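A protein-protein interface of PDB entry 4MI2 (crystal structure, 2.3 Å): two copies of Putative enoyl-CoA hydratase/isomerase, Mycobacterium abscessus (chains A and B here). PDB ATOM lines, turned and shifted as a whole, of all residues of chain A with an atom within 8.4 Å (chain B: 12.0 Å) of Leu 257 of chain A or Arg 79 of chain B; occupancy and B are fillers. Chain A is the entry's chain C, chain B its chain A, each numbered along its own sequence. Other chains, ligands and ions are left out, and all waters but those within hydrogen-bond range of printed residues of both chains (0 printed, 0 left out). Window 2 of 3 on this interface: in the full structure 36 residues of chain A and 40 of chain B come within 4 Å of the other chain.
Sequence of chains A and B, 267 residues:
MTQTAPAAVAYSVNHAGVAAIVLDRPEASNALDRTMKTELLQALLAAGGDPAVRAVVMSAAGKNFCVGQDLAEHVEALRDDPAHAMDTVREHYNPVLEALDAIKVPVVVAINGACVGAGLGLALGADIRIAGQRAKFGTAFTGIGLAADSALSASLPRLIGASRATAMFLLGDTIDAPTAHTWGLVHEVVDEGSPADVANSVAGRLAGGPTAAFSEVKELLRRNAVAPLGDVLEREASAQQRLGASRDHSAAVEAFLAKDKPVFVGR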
ATOM      1  N   GLY A 244     -11.438  16.530  -6.565  1.00  0.00           N
ATOM      2  CA  GLY A 244     -11.104  15.714  -7.732  1.00  0.00           C
ATOM      3  C   GLY A 244      -9.703  15.129  -7.673  1.00  0.00           C
ATOM      4  O   GLY A 244      -9.425  14.104  -8.290  1.00  0.00           O
ATOM      5  N   SER A 250     -10.702   9.219  -6.285  1.00  0.00           N
ATOM      6  CA  SER A 250     -10.182   8.191  -7.185  1.00  0.00           C
ATOM      7  C   SER A 250     -10.650   6.809  -6.758  1.00  0.00           C
ATOM      8  O   SER A 250     -11.134   6.053  -7.590  1.00  0.00           O
ATOM      9  CB  SER A 250      -8.662   8.243  -7.309  1.00  0.00           C
ATOM     10  OG  SER A 250      -8.309   9.239  -8.256  1.00  0.00           O
ATOM     11  N   ALA A 251     -10.533   6.498  -5.469  1.00  0.00           N
ATOM     12  CA  ALA A 251     -11.031   5.214  -4.947  1.00  0.00           C
ATOM     13  C   ALA A 251     -12.529   5.006  -5.256  1.00  0.00           C
ATOM     14  O   ALA A 251     -12.953   3.913  -5.636  1.00  0.00           O
ATOM     15  CB  ALA A 251     -10.776   5.108  -3.450  1.00  0.00           C
ATOM     16  N   ALA A 252     -13.323   6.062  -5.120  1.00  0.00           N
ATOM     17  CA  ALA A 252     -14.750   5.960  -5.368  1.00  0.00           C
ATOM     18  C   ALA A 252     -15.057   5.758  -6.855  1.00  0.00           C
ATOM     19  O   ALA A 252     -15.999   5.027  -7.205  1.00  0.00           O
ATOM     20  CB  ALA A 252     -15.482   7.176  -4.825  1.00  0.00           C
ATOM     21  N   VAL A 253     -14.265   6.386  -7.722  1.00  0.00           N
ATOM     22  CA  VAL A 253     -14.471   6.244  -9.154  1.00  0.00           C
ATOM     23  C   VAL A 253     -14.199   4.801  -9.577  1.00  0.00           C
ATOM     24  O   VAL A 253     -15.003   4.222 -10.303  1.00  0.00           O
ATOM     25  CB  VAL A 253     -13.611   7.222  -9.979  1.00  0.00           C
ATOM     26  CG1 VAL A 253     -13.714   6.901 -11.463  1.00  0.00           C
ATOM     27  CG2 VAL A 253     -14.048   8.667  -9.726  1.00  0.00           C
ATOM     28  N   GLU A 254     -13.093   4.215  -9.118  1.00  0.00           N
ATOM     29  CA  GLU A 254     -12.817   2.810  -9.472  1.00  0.00           C
ATOM     30  C   GLU A 254     -13.785   1.835  -8.805  1.00  0.00           C
ATOM     31  O   GLU A 254     -14.136   0.845  -9.410  1.00  0.00           O
ATOM     32  CB  GLU A 254     -11.344   2.400  -9.292  1.00  0.00           C
ATOM     33  CG  GLU A 254     -10.676   2.746  -7.970  1.00  0.00           C
ATOM     34  CD  GLU A 254      -9.201   3.123  -8.128  1.00  0.00           C
ATOM     35  OE1 GLU A 254      -8.462   3.077  -7.113  1.00  0.00           O
ATOM     36  OE2 GLU A 254      -8.777   3.467  -9.260  1.00  0.00           O
ATOM     37  N   ALA A 255     -14.261   2.141  -7.602  1.00  0.00           N
ATOM     38  CA  ALA A 255     -15.336   1.360  -6.994  1.00  0.00           C
ATOM     39  C   ALA A 255     -16.627   1.417  -7.827  1.00  0.00           C
ATOM     40  O   ALA A 255     -17.251   0.390  -8.061  1.00  0.00           O
ATOM     41  CB  ALA A 255     -15.603   1.818  -5.566  1.00  0.00           C
ATOM     42  N   PHE A 256     -17.012   2.612  -8.276  1.00  0.00           N
ATOM     43  CA  PHE A 256     -18.211   2.798  -9.127  1.00  0.00           C
ATOM     44  C   PHE A 256     -18.134   2.037 -10.455  1.00  0.00           C
ATOM     45  O   PHE A 256     -19.140   1.522 -10.937  1.00  0.00           O
ATOM     46  CB  PHE A 256     -18.445   4.288  -9.442  1.00  0.00           C
ATOM     47  CG  PHE A 256     -19.250   5.027  -8.402  1.00  0.00           C
ATOM     48  CD1 PHE A 256     -20.267   5.893  -8.788  1.00  0.00           C
ATOM     49  CD2 PHE A 256     -18.988   4.873  -7.040  1.00  0.00           C
ATOM     50  CE1 PHE A 256     -21.006   6.589  -7.839  1.00  0.00           C
ATOM     51  CE2 PHE A 256     -19.729   5.562  -6.087  1.00  0.00           C
ATOM     52  CZ  PHE A 256     -20.736   6.423  -6.487  1.00  0.00           C
ATOM     53  N   LEU A 257     -16.946   1.980 -11.047  1.00  0.00           N
ATOM     54  CA  LEU A 257     -16.735   1.226 -12.284  1.00  0.00           C
ATOM     55  C   LEU A 257     -17.028  -0.264 -12.090  1.00  0.00           C
ATOM     56  O   LEU A 257     -17.510  -0.923 -13.000  1.00  0.00           O
ATOM     57  CB  LEU A 257     -15.305   1.426 -12.803  1.00  0.00           C
ATOM     58  CG  LEU A 257     -15.034   2.752 -13.522  1.00  0.00           C
ATOM     59  CD1 LEU A 257     -13.534   3.000 -13.623  1.00  0.00           C
ATOM     60  CD2 LEU A 257     -15.676   2.762 -14.905  1.00  0.00           C
ATOM     61  N   ALA A 258     -16.753  -0.771 -10.893  1.00  0.00           N
ATOM     62  CA  ALA A 258     -17.070  -2.151 -10.538  1.00  0.00           C
ATOM     63  C   ALA A 258     -18.444  -2.280  -9.855  1.00  0.00           C
ATOM     64  O   ALA A 258     -18.806  -3.363  -9.389  1.00  0.00           O
ATOM     65  CB  ALA A 258     -15.977  -2.709  -9.636  1.00  0.00           C
ATOM     66  N   LYS A 259     -19.203  -1.183  -9.806  1.00  0.00           N
ATOM     67  CA  LYS A 259     -20.479  -1.124  -9.074  1.00  0.00           C
ATOM     68  C   LYS A 259     -20.342  -1.491  -7.588  1.00  0.00           C
ATOM     69  O   LYS A 259     -21.246  -2.091  -7.017  1.00  0.00           O
ATOM     70  CB  LYS A 259     -21.540  -2.014  -9.745  1.00  0.00           C
ATOM     71  CG  LYS A 259     -21.785  -1.686 -11.209  1.00  0.00           C
ATOM     72  CD  LYS A 259     -22.663  -2.734 -11.870  1.00  0.00           C
ATOM     73  CE  LYS A 259     -22.895  -2.420 -13.340  1.00  0.00           C
ATOM     74  NZ  LYS A 259     -23.653  -3.501 -14.034  1.00  0.00           N
ATOM     75  N   ASP A 260     -19.219  -1.124  -6.969  1.00  0.00           N
ATOM     76  CA  ASP A 260     -19.028  -1.300  -5.515  1.00  0.00           C
ATOM     77  C   ASP A 260     -19.307  -0.012  -4.761  1.00  0.00           C
ATOM     78  O   ASP A 260     -19.290   1.072  -5.342  1.00  0.00           O
ATOM     79  CB  ASP A 260     -17.587  -1.701  -5.181  1.00  0.00           C
ATOM     80  CG  ASP A 260     -17.296  -3.136  -5.486  1.00  0.00           C
ATOM     81  OD1 ASP A 260     -18.112  -3.769  -6.191  1.00  0.00           O
ATOM     82  OD2 ASP A 260     -16.241  -3.636  -5.018  1.00  0.00           O
ATOM     83  N   LYS A 261     -19.549  -0.146  -3.461  1.00  0.00           N
ATOM     84  CA  LYS A 261     -19.497   0.993  -2.550  1.00  0.00           C
ATOM     85  C   LYS A 261     -18.025   1.169  -2.213  1.00  0.00           C
ATOM     86  O   LYS A 261     -17.338   0.191  -1.941  1.00  0.00           O
ATOM     87  CB  LYS A 261     -20.326   0.753  -1.277  1.00  0.00           C
ATOM     88  N   ARG B  34     -20.348  15.899 -22.815  1.00  0.00           N
ATOM     89  CA  ARG B  34     -20.099  17.224 -23.413  1.00  0.00           C
ATOM     90  C   ARG B  34     -21.169  17.623 -24.436  1.00  0.00           C
ATOM     91  O   ARG B  34     -21.649  18.754 -24.427  1.00  0.00           O
ATOM     92  CB  ARG B  34     -18.695  17.303 -24.040  1.00  0.00           C
ATOM     93  CG  ARG B  34     -17.582  17.553 -23.028  1.00  0.00           C
ATOM     94  CD  ARG B  34     -16.220  17.764 -23.689  1.00  0.00           C
ATOM     95  NE  ARG B  34     -15.751  16.556 -24.368  1.00  0.00           N
ATOM     96  CZ  ARG B  34     -15.120  15.531 -23.782  1.00  0.00           C
ATOM     97  NH1 ARG B  34     -14.848  15.540 -22.479  1.00  0.00           N
ATOM     98  NH2 ARG B  34     -14.751  14.478 -24.509  1.00  0.00           N
ATOM     99  N   GLN B  69     -23.503  13.855 -14.187  1.00  0.00           N
ATOM    100  CA  GLN B  69     -22.305  13.732 -15.012  1.00  0.00           C
ATOM    101  C   GLN B  69     -22.131  12.331 -15.616  1.00  0.00           C
ATOM    102  O   GLN B  69     -22.286  11.330 -14.933  1.00  0.00           O
ATOM    103  CB  GLN B  69     -21.069  14.109 -14.189  1.00  0.00           C
ATOM    104  CG  GLN B  69     -19.732  13.848 -14.875  1.00  0.00           C
ATOM    105  CD  GLN B  69     -19.574  14.601 -16.183  1.00  0.00           C
ATOM    106  OE1 GLN B  69     -19.875  15.792 -16.279  1.00  0.00           O
ATOM    107  NE2 GLN B  69     -19.072  13.911 -17.193  1.00  0.00           N
ATOM    108  N   ASP B  70     -21.823  12.284 -16.909  1.00  0.00           N
ATOM    109  CA  ASP B  70     -21.497  11.031 -17.593  1.00  0.00           C
ATOM    110  C   ASP B  70     -20.252  10.435 -16.958  1.00  0.00           C
ATOM    111  O   ASP B  70     -19.203  11.088 -16.905  1.00  0.00           O
ATOM    112  CB  ASP B  70     -21.244  11.290 -19.080  1.00  0.00           C
ATOM    113  CG  ASP B  70     -21.072  10.008 -19.881  1.00  0.00           C
ATOM    114  OD1 ASP B  70     -22.097   9.394 -20.245  1.00  0.00           O
ATOM    115  OD2 ASP B  70     -19.920   9.623 -20.159  1.00  0.00           O
ATOM    116  N   LEU B  71     -20.371   9.206 -16.471  1.00  0.00           N
ATOM    117  CA  LEU B  71     -19.278   8.564 -15.750  1.00  0.00           C
ATOM    118  C   LEU B  71     -18.051   8.312 -16.642  1.00  0.00           C
ATOM    119  O   LEU B  71     -16.931   8.652 -16.264  1.00  0.00           O
ATOM    120  CB  LEU B  71     -19.764   7.258 -15.121  1.00  0.00           C
ATOM    121  CG  LEU B  71     -18.715   6.383 -14.431  1.00  0.00           C
ATOM    122  CD1 LEU B  71     -17.983   7.152 -13.342  1.00  0.00           C
ATOM    123  CD2 LEU B  71     -19.382   5.139 -13.863  1.00  0.00           C
ATOM    124  N   ALA B  72     -18.264   7.740 -17.823  1.00  0.00           N
ATOM    125  CA  ALA B  72     -17.152   7.363 -18.699  1.00  0.00           C
ATOM    126  C   ALA B  72     -16.329   8.577 -19.089  1.00  0.00           C
ATOM    127  O   ALA B  72     -15.101   8.549 -19.051  1.00  0.00           O
ATOM    128  CB  ALA B  72     -17.659   6.650 -19.951  1.00  0.00           C
ATOM    129  N   GLU B  73     -17.012   9.647 -19.462  1.00  0.00           N
ATOM    130  CA  GLU B  73     -16.336  10.883 -19.825  1.00  0.00           C
ATOM    131  C   GLU B  73     -15.546  11.438 -18.638  1.00  0.00           C
ATOM    132  O   GLU B  73     -14.444  11.961 -18.797  1.00  0.00           O
ATOM    133  CB  GLU B  73     -17.367  11.898 -20.285  1.00  0.00           C
ATOM    134  CG  GLU B  73     -16.804  13.086 -21.011  1.00  0.00           C
ATOM    135  CD  GLU B  73     -17.914  13.893 -21.660  1.00  0.00           C
ATOM    136  OE1 GLU B  73     -18.228  13.619 -22.842  1.00  0.00           O
ATOM    137  OE2 GLU B  73     -18.489  14.763 -20.968  1.00  0.00           O
ATOM    138  N   HIS B  74     -16.108  11.313 -17.444  1.00  0.00           N
ATOM    139  CA  HIS B  74     -15.398  11.708 -16.249  1.00  0.00           C
ATOM    140  C   HIS B  74     -14.161  10.849 -15.975  1.00  0.00           C
ATOM    141  O   HIS B  74     -13.134  11.364 -15.546  1.00  0.00           O
ATOM    142  CB  HIS B  74     -16.306  11.674 -15.023  1.00  0.00           C
ATOM    143  CG  HIS B  74     -15.596  12.096 -13.789  1.00  0.00           C
ATOM    144  ND1 HIS B  74     -15.253  13.408 -13.544  1.00  0.00           N
ATOM    145  CD2 HIS B  74     -15.058  11.370 -12.786  1.00  0.00           C
ATOM    146  CE1 HIS B  74     -14.583  13.477 -12.409  1.00  0.00           C
ATOM    147  NE2 HIS B  74     -14.453  12.254 -11.930  1.00  0.00           N
ATOM    148  N   VAL B  75     -14.280   9.540 -16.186  1.00  0.00           N
ATOM    149  CA  VAL B  75     -13.149   8.621 -16.038  1.00  0.00           C
ATOM    150  C   VAL B  75     -11.994   9.028 -16.959  1.00  0.00           C
ATOM    151  O   VAL B  75     -10.834   9.016 -16.535  1.00  0.00           O
ATOM    152  CB  VAL B  75     -13.559   7.148 -16.324  1.00  0.00           C
ATOM    153  CG1 VAL B  75     -12.338   6.244 -16.456  1.00  0.00           C
ATOM    154  CG2 VAL B  75     -14.491   6.625 -15.234  1.00  0.00           C
ATOM    155  N   GLU B  76     -12.310   9.395 -18.204  1.00  0.00           N
ATOM    156  CA  GLU B  76     -11.281   9.793 -19.171  1.00  0.00           C
ATOM    157  C   GLU B  76     -10.519  11.030 -18.680  1.00  0.00           C
ATOM    158  O   GLU B  76      -9.287  11.050 -18.685  1.00  0.00           O
ATOM    159  CB  GLU B  76     -11.883  10.029 -20.560  1.00  0.00           C
ATOM    160  N   ALA B  77     -11.260  12.042 -18.228  1.00  0.00           N
ATOM    161  CA  ALA B  77     -10.663  13.278 -17.705  1.00  0.00           C
ATOM    162  C   ALA B  77      -9.802  13.034 -16.466  1.00  0.00           C
ATOM    163  O   ALA B  77      -8.756  13.657 -16.286  1.00  0.00           O
ATOM    164  CB  ALA B  77     -11.751  14.295 -17.385  1.00  0.00           C
ATOM    165  N   LEU B  78     -10.257  12.123 -15.618  1.00  0.00           N
ATOM    166  CA  LEU B  78      -9.591  11.841 -14.357  1.00  0.00           C
ATOM    167  C   LEU B  78      -8.284  11.101 -14.599  1.00  0.00           C
ATOM    168  O   LEU B  78      -7.261  11.417 -13.986  1.00  0.00           O
ATOM    169  CB  LEU B  78     -10.515  11.029 -13.451  1.00  0.00           C
ATOM    170  CG  LEU B  78     -10.094  10.821 -12.003  1.00  0.00           C
ATOM    171  CD1 LEU B  78      -9.902  12.137 -11.277  1.00  0.00           C
ATOM    172  CD2 LEU B  78     -11.141   9.963 -11.297  1.00  0.00           C
ATOM    173  N   ARG B  79      -8.313  10.135 -15.509  1.00  0.00           N
ATOM    174  CA  ARG B  79      -7.101   9.409 -15.885  1.00  0.00           C
ATOM    175  C   ARG B  79      -6.132  10.285 -16.669  1.00  0.00           C
ATOM    176  O   ARG B  79      -4.922  10.098 -16.582  1.00  0.00           O
ATOM    177  CB  ARG B  79      -7.449   8.145 -16.673  1.00  0.00           C
ATOM    178  CG  ARG B  79      -7.983   7.046 -15.773  1.00  0.00           C
ATOM    179  CD  ARG B  79      -8.475   5.836 -16.551  1.00  0.00           C
ATOM    180  NE  ARG B  79      -8.929   4.782 -15.639  1.00  0.00           N
ATOM    181  CZ  ARG B  79      -9.721   3.765 -15.981  1.00  0.00           C
ATOM    182  NH1 ARG B  79     -10.173   3.639 -17.228  1.00  0.00           N
ATOM    183  NH2 ARG B  79     -10.069   2.868 -15.062  1.00  0.00           N
ATOM    184  N   ASP B  80      -6.671  11.250 -17.407  1.00  0.00           N
ATOM    185  CA  ASP B  80      -5.868  12.139 -18.236  1.00  0.00           C
ATOM    186  C   ASP B  80      -5.166  13.224 -17.422  1.00  0.00           C
ATOM    187  O   ASP B  80      -4.013  13.533 -17.691  1.00  0.00           O
ATOM    188  CB  ASP B  80      -6.740  12.794 -19.316  1.00  0.00           C
ATOM    189  CG  ASP B  80      -6.005  13.870 -20.084  1.00  0.00           C
ATOM    190  OD1 ASP B  80      -6.492  15.022 -20.118  1.00  0.00           O
ATOM    191  OD2 ASP B  80      -4.927  13.565 -20.635  1.00  0.00           O
ATOM    192  N   ASP B  81      -5.866  13.802 -16.444  1.00  0.00           N
ATOM    193  CA  ASP B  81      -5.321  14.899 -15.647  1.00  0.00           C
ATOM    194  C   ASP B  81      -6.136  15.146 -14.361  1.00  0.00           C
ATOM    195  O   ASP B  81      -7.017  16.013 -14.329  1.00  0.00           O
ATOM    196  CB  ASP B  81      -5.280  16.164 -16.509  1.00  0.00           C
ATOM    197  CG  ASP B  81      -4.593  17.317 -15.826  1.00  0.00           C
ATOM    198  OD1 ASP B  81      -4.085  17.147 -14.691  1.00  0.00           O
ATOM    199  OD2 ASP B  81      -4.572  18.402 -16.438  1.00  0.00           O
ATOM    200  N   PRO B  82      -5.847  14.378 -13.293  1.00  0.00           N
ATOM    201  CA  PRO B  82      -6.682  14.428 -12.074  1.00  0.00           C
ATOM    202  C   PRO B  82      -6.790  15.815 -11.419  1.00  0.00           C
ATOM    203  O   PRO B  82      -7.845  16.169 -10.898  1.00  0.00           O
ATOM    204  CB  PRO B  82      -6.015  13.417 -11.124  1.00  0.00           C
ATOM    205  CG  PRO B  82      -4.693  13.091 -11.726  1.00  0.00           C
ATOM    206  CD  PRO B  82      -4.774  13.372 -13.194  1.00  0.00           C
ATOM    207  N   ALA B  83      -5.720  16.597 -11.469  1.00  0.00           N
ATOM    208  CA  ALA B  83      -5.740  17.941 -10.918  1.00  0.00           C
ATOM    209  C   ALA B  83      -6.680  18.880 -11.688  1.00  0.00           C
ATOM    210  O   ALA B  83      -6.975  19.979 -11.205  1.00  0.00           O
ATOM    211  CB  ALA B  83      -4.326  18.516 -10.900  1.00  0.00           C
ATOM    212  N   HIS B  84      -7.126  18.470 -12.882  1.00  0.00           N
ATOM    213  CA  HIS B  84      -8.002  19.312 -13.707  1.00  0.00           C
ATOM    214  C   HIS B  84      -9.263  18.616 -14.202  1.00  0.00           C
ATOM    215  O   HIS B  84      -9.908  19.097 -15.132  1.00  0.00           O
ATOM    216  CB  HIS B  84      -7.225  19.875 -14.898  1.00  0.00           C
ATOM    217  CG  HIS B  84      -6.059  20.730 -14.504  1.00  0.00           C
ATOM    218  ND1 HIS B  84      -4.786  20.532 -14.998  1.00  0.00           N
ATOM    219  CD2 HIS B  84      -5.973  21.784 -13.658  1.00  0.00           C
ATOM    220  CE1 HIS B  84      -3.967  21.430 -14.479  1.00  0.00           C
ATOM    221  NE2 HIS B  84      -4.663  22.200 -13.661  1.00  0.00           N
ATOM    222  N   ALA B  85      -9.645  17.516 -13.555  1.00  0.00           N
ATOM    223  CA  ALA B  85     -10.750  16.692 -14.040  1.00  0.00           C
ATOM    224  C   ALA B  85     -12.120  17.344 -13.850  1.00  0.00           C
ATOM    225  O   ALA B  85     -13.102  16.902 -14.455  1.00  0.00           O
ATOM    226  CB  ALA B  85     -10.723  15.333 -13.369  1.00  0.00           C
ATOM    227  N   MET B  86     -12.177  18.378 -13.009  1.00  0.00           N
ATOM    228  CA  MET B  86     -13.406  19.113 -12.758  1.00  0.00           C
ATOM    229  C   MET B  86     -13.482  20.438 -13.518  1.00  0.00           C
ATOM    230  O   MET B  86     -14.282  21.291 -13.176  1.00  0.00           O
ATOM    231  CB  MET B  86     -13.575  19.366 -11.263  1.00  0.00           C
ATOM    232  CG  MET B  86     -13.328  18.164 -10.378  1.00  0.00           C
ATOM    233  SD  MET B  86     -14.309  16.723 -10.795  1.00  0.00           S
ATOM    234  CE  MET B  86     -16.004  17.308 -10.802  1.00  0.00           C
ATOM    235  N   ASP B  87     -12.657  20.608 -14.545  1.00  0.00           N
ATOM    236  CA  ASP B  87     -12.766  21.758 -15.457  1.00  0.00           C
ATOM    237  C   ASP B  87     -14.201  21.937 -15.972  1.00  0.00           C
ATOM    238  O   ASP B  87     -14.662  23.065 -16.164  1.00  0.00           O
ATOM    239  CB  ASP B  87     -11.818  21.599 -16.664  1.00  0.00           C
ATOM    240  CG  ASP B  87     -10.397  22.094 -16.383  1.00  0.00           C
ATOM    241  OD1 ASP B  87     -10.143  22.699 -15.323  1.00  0.00           O
ATOM    242  OD2 ASP B  87      -9.522  21.886 -17.243  1.00  0.00           O
ATOM    243  N   GLY B 143     -21.303  10.512  -2.330  1.00  0.00           N
ATOM    244  CA  GLY B 143     -21.164   9.103  -2.669  1.00  0.00           C
ATOM    245  C   GLY B 143     -19.895   8.793  -3.442  1.00  0.00           C
ATOM    246  O   GLY B 143     -19.309   7.737  -3.264  1.00  0.00           O
ATOM    247  N   ILE B 144     -19.458   9.729  -4.284  1.00  0.00           N
ATOM    248  CA  ILE B 144     -18.248   9.561  -5.080  1.00  0.00           C
ATOM    249  C   ILE B 144     -17.106  10.473  -4.575  1.00  0.00           C
ATOM    250  O   ILE B 144     -16.168  10.775  -5.300  1.00  0.00           O
ATOM    251  CB  ILE B 144     -18.577   9.759  -6.586  1.00  0.00           C
ATOM    252  CG1 ILE B 144     -17.584   9.014  -7.486  1.00  0.00           C
ATOM    253  CG2 ILE B 144     -18.645  11.227  -6.977  1.00  0.00           C
ATOM    254  CD1 ILE B 144     -18.006   9.003  -8.940  1.00  0.00           C
ATOM    255  N   GLY B 145     -17.189  10.896  -3.316  1.00  0.00           N
ATOM    256  CA  GLY B 145     -16.113  11.661  -2.678  1.00  0.00           C
ATOM    257  C   GLY B 145     -15.973  13.101  -3.127  1.00  0.00           C
ATOM    258  O   GLY B 145     -14.905  13.701  -2.973  1.00  0.00           O
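No position is printed for both chains. Of the 8 pairs that touch across the chains among the printed residues, none has its exchanged pair printed and touching as well.
Printed residues of chain A that touch a printed residue of chain B: Gly 244, Ala 252, Val 253, Phe 256 and Leu 257. Hydrophobic or aromatic side chains of chain A that line the printed part of chain B: Ala 252, Val 253, Phe 256 and Leu 257.
Among the printed residues, merely in contact across the chains: Val 253 of chain A with Leu 78 of chain B, Phe 256 of chain A with Gly 143 of chain B, Gly 244 of chain A with Leu 78 of chain B, Ala 252 of chain A with Ile 144 of chain B, Gly 244 of chain A with Pro 82 of chain B, Leu 257 of chain A with Arg 79 of chain B, Phe 256 of chain A with Ile 144 of chain B and Val 253 of chain A with Val 75 of chain B.
Leu 257 of chain A touches one residue of chain B. Of the printed residues of chain A, Arg 79 of chain B touches Leu 257. Val 253 of chain A touches two residues of chain B. Of chain B, only Gly 143 and Ile 144 come within 4 Å of Phe 256 of chain A. No residue of chain B comes within 4 Å of Lys 259 of chain A. No residue of chain B comes within 4 Å of Asp 260 of chain A. Of the printed residues of chain A, Leu 78 of chain B touches Gly 244 and Val 253. Of the printed residues of chain B, Ala 252 of chain A touches Ile 144. Printed residues of chain B within 4 Å of Gly 244 of chain A: Leu 78 (3.6 Å) and Pro 82 (3.7 Å). Printed residues of chain A within 4 Å of Ile 144 of chain B: Ala 252 and Phe 256. Of the printed residues of chain A, Pro 82 of chain B touches Gly 244. Glu 76 of chain B touches none of the printed residues of chain A. The nearest printed residue of chain A that does not touch Ile 144 of chain B is Val 253 of chain A (4.05 Å).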
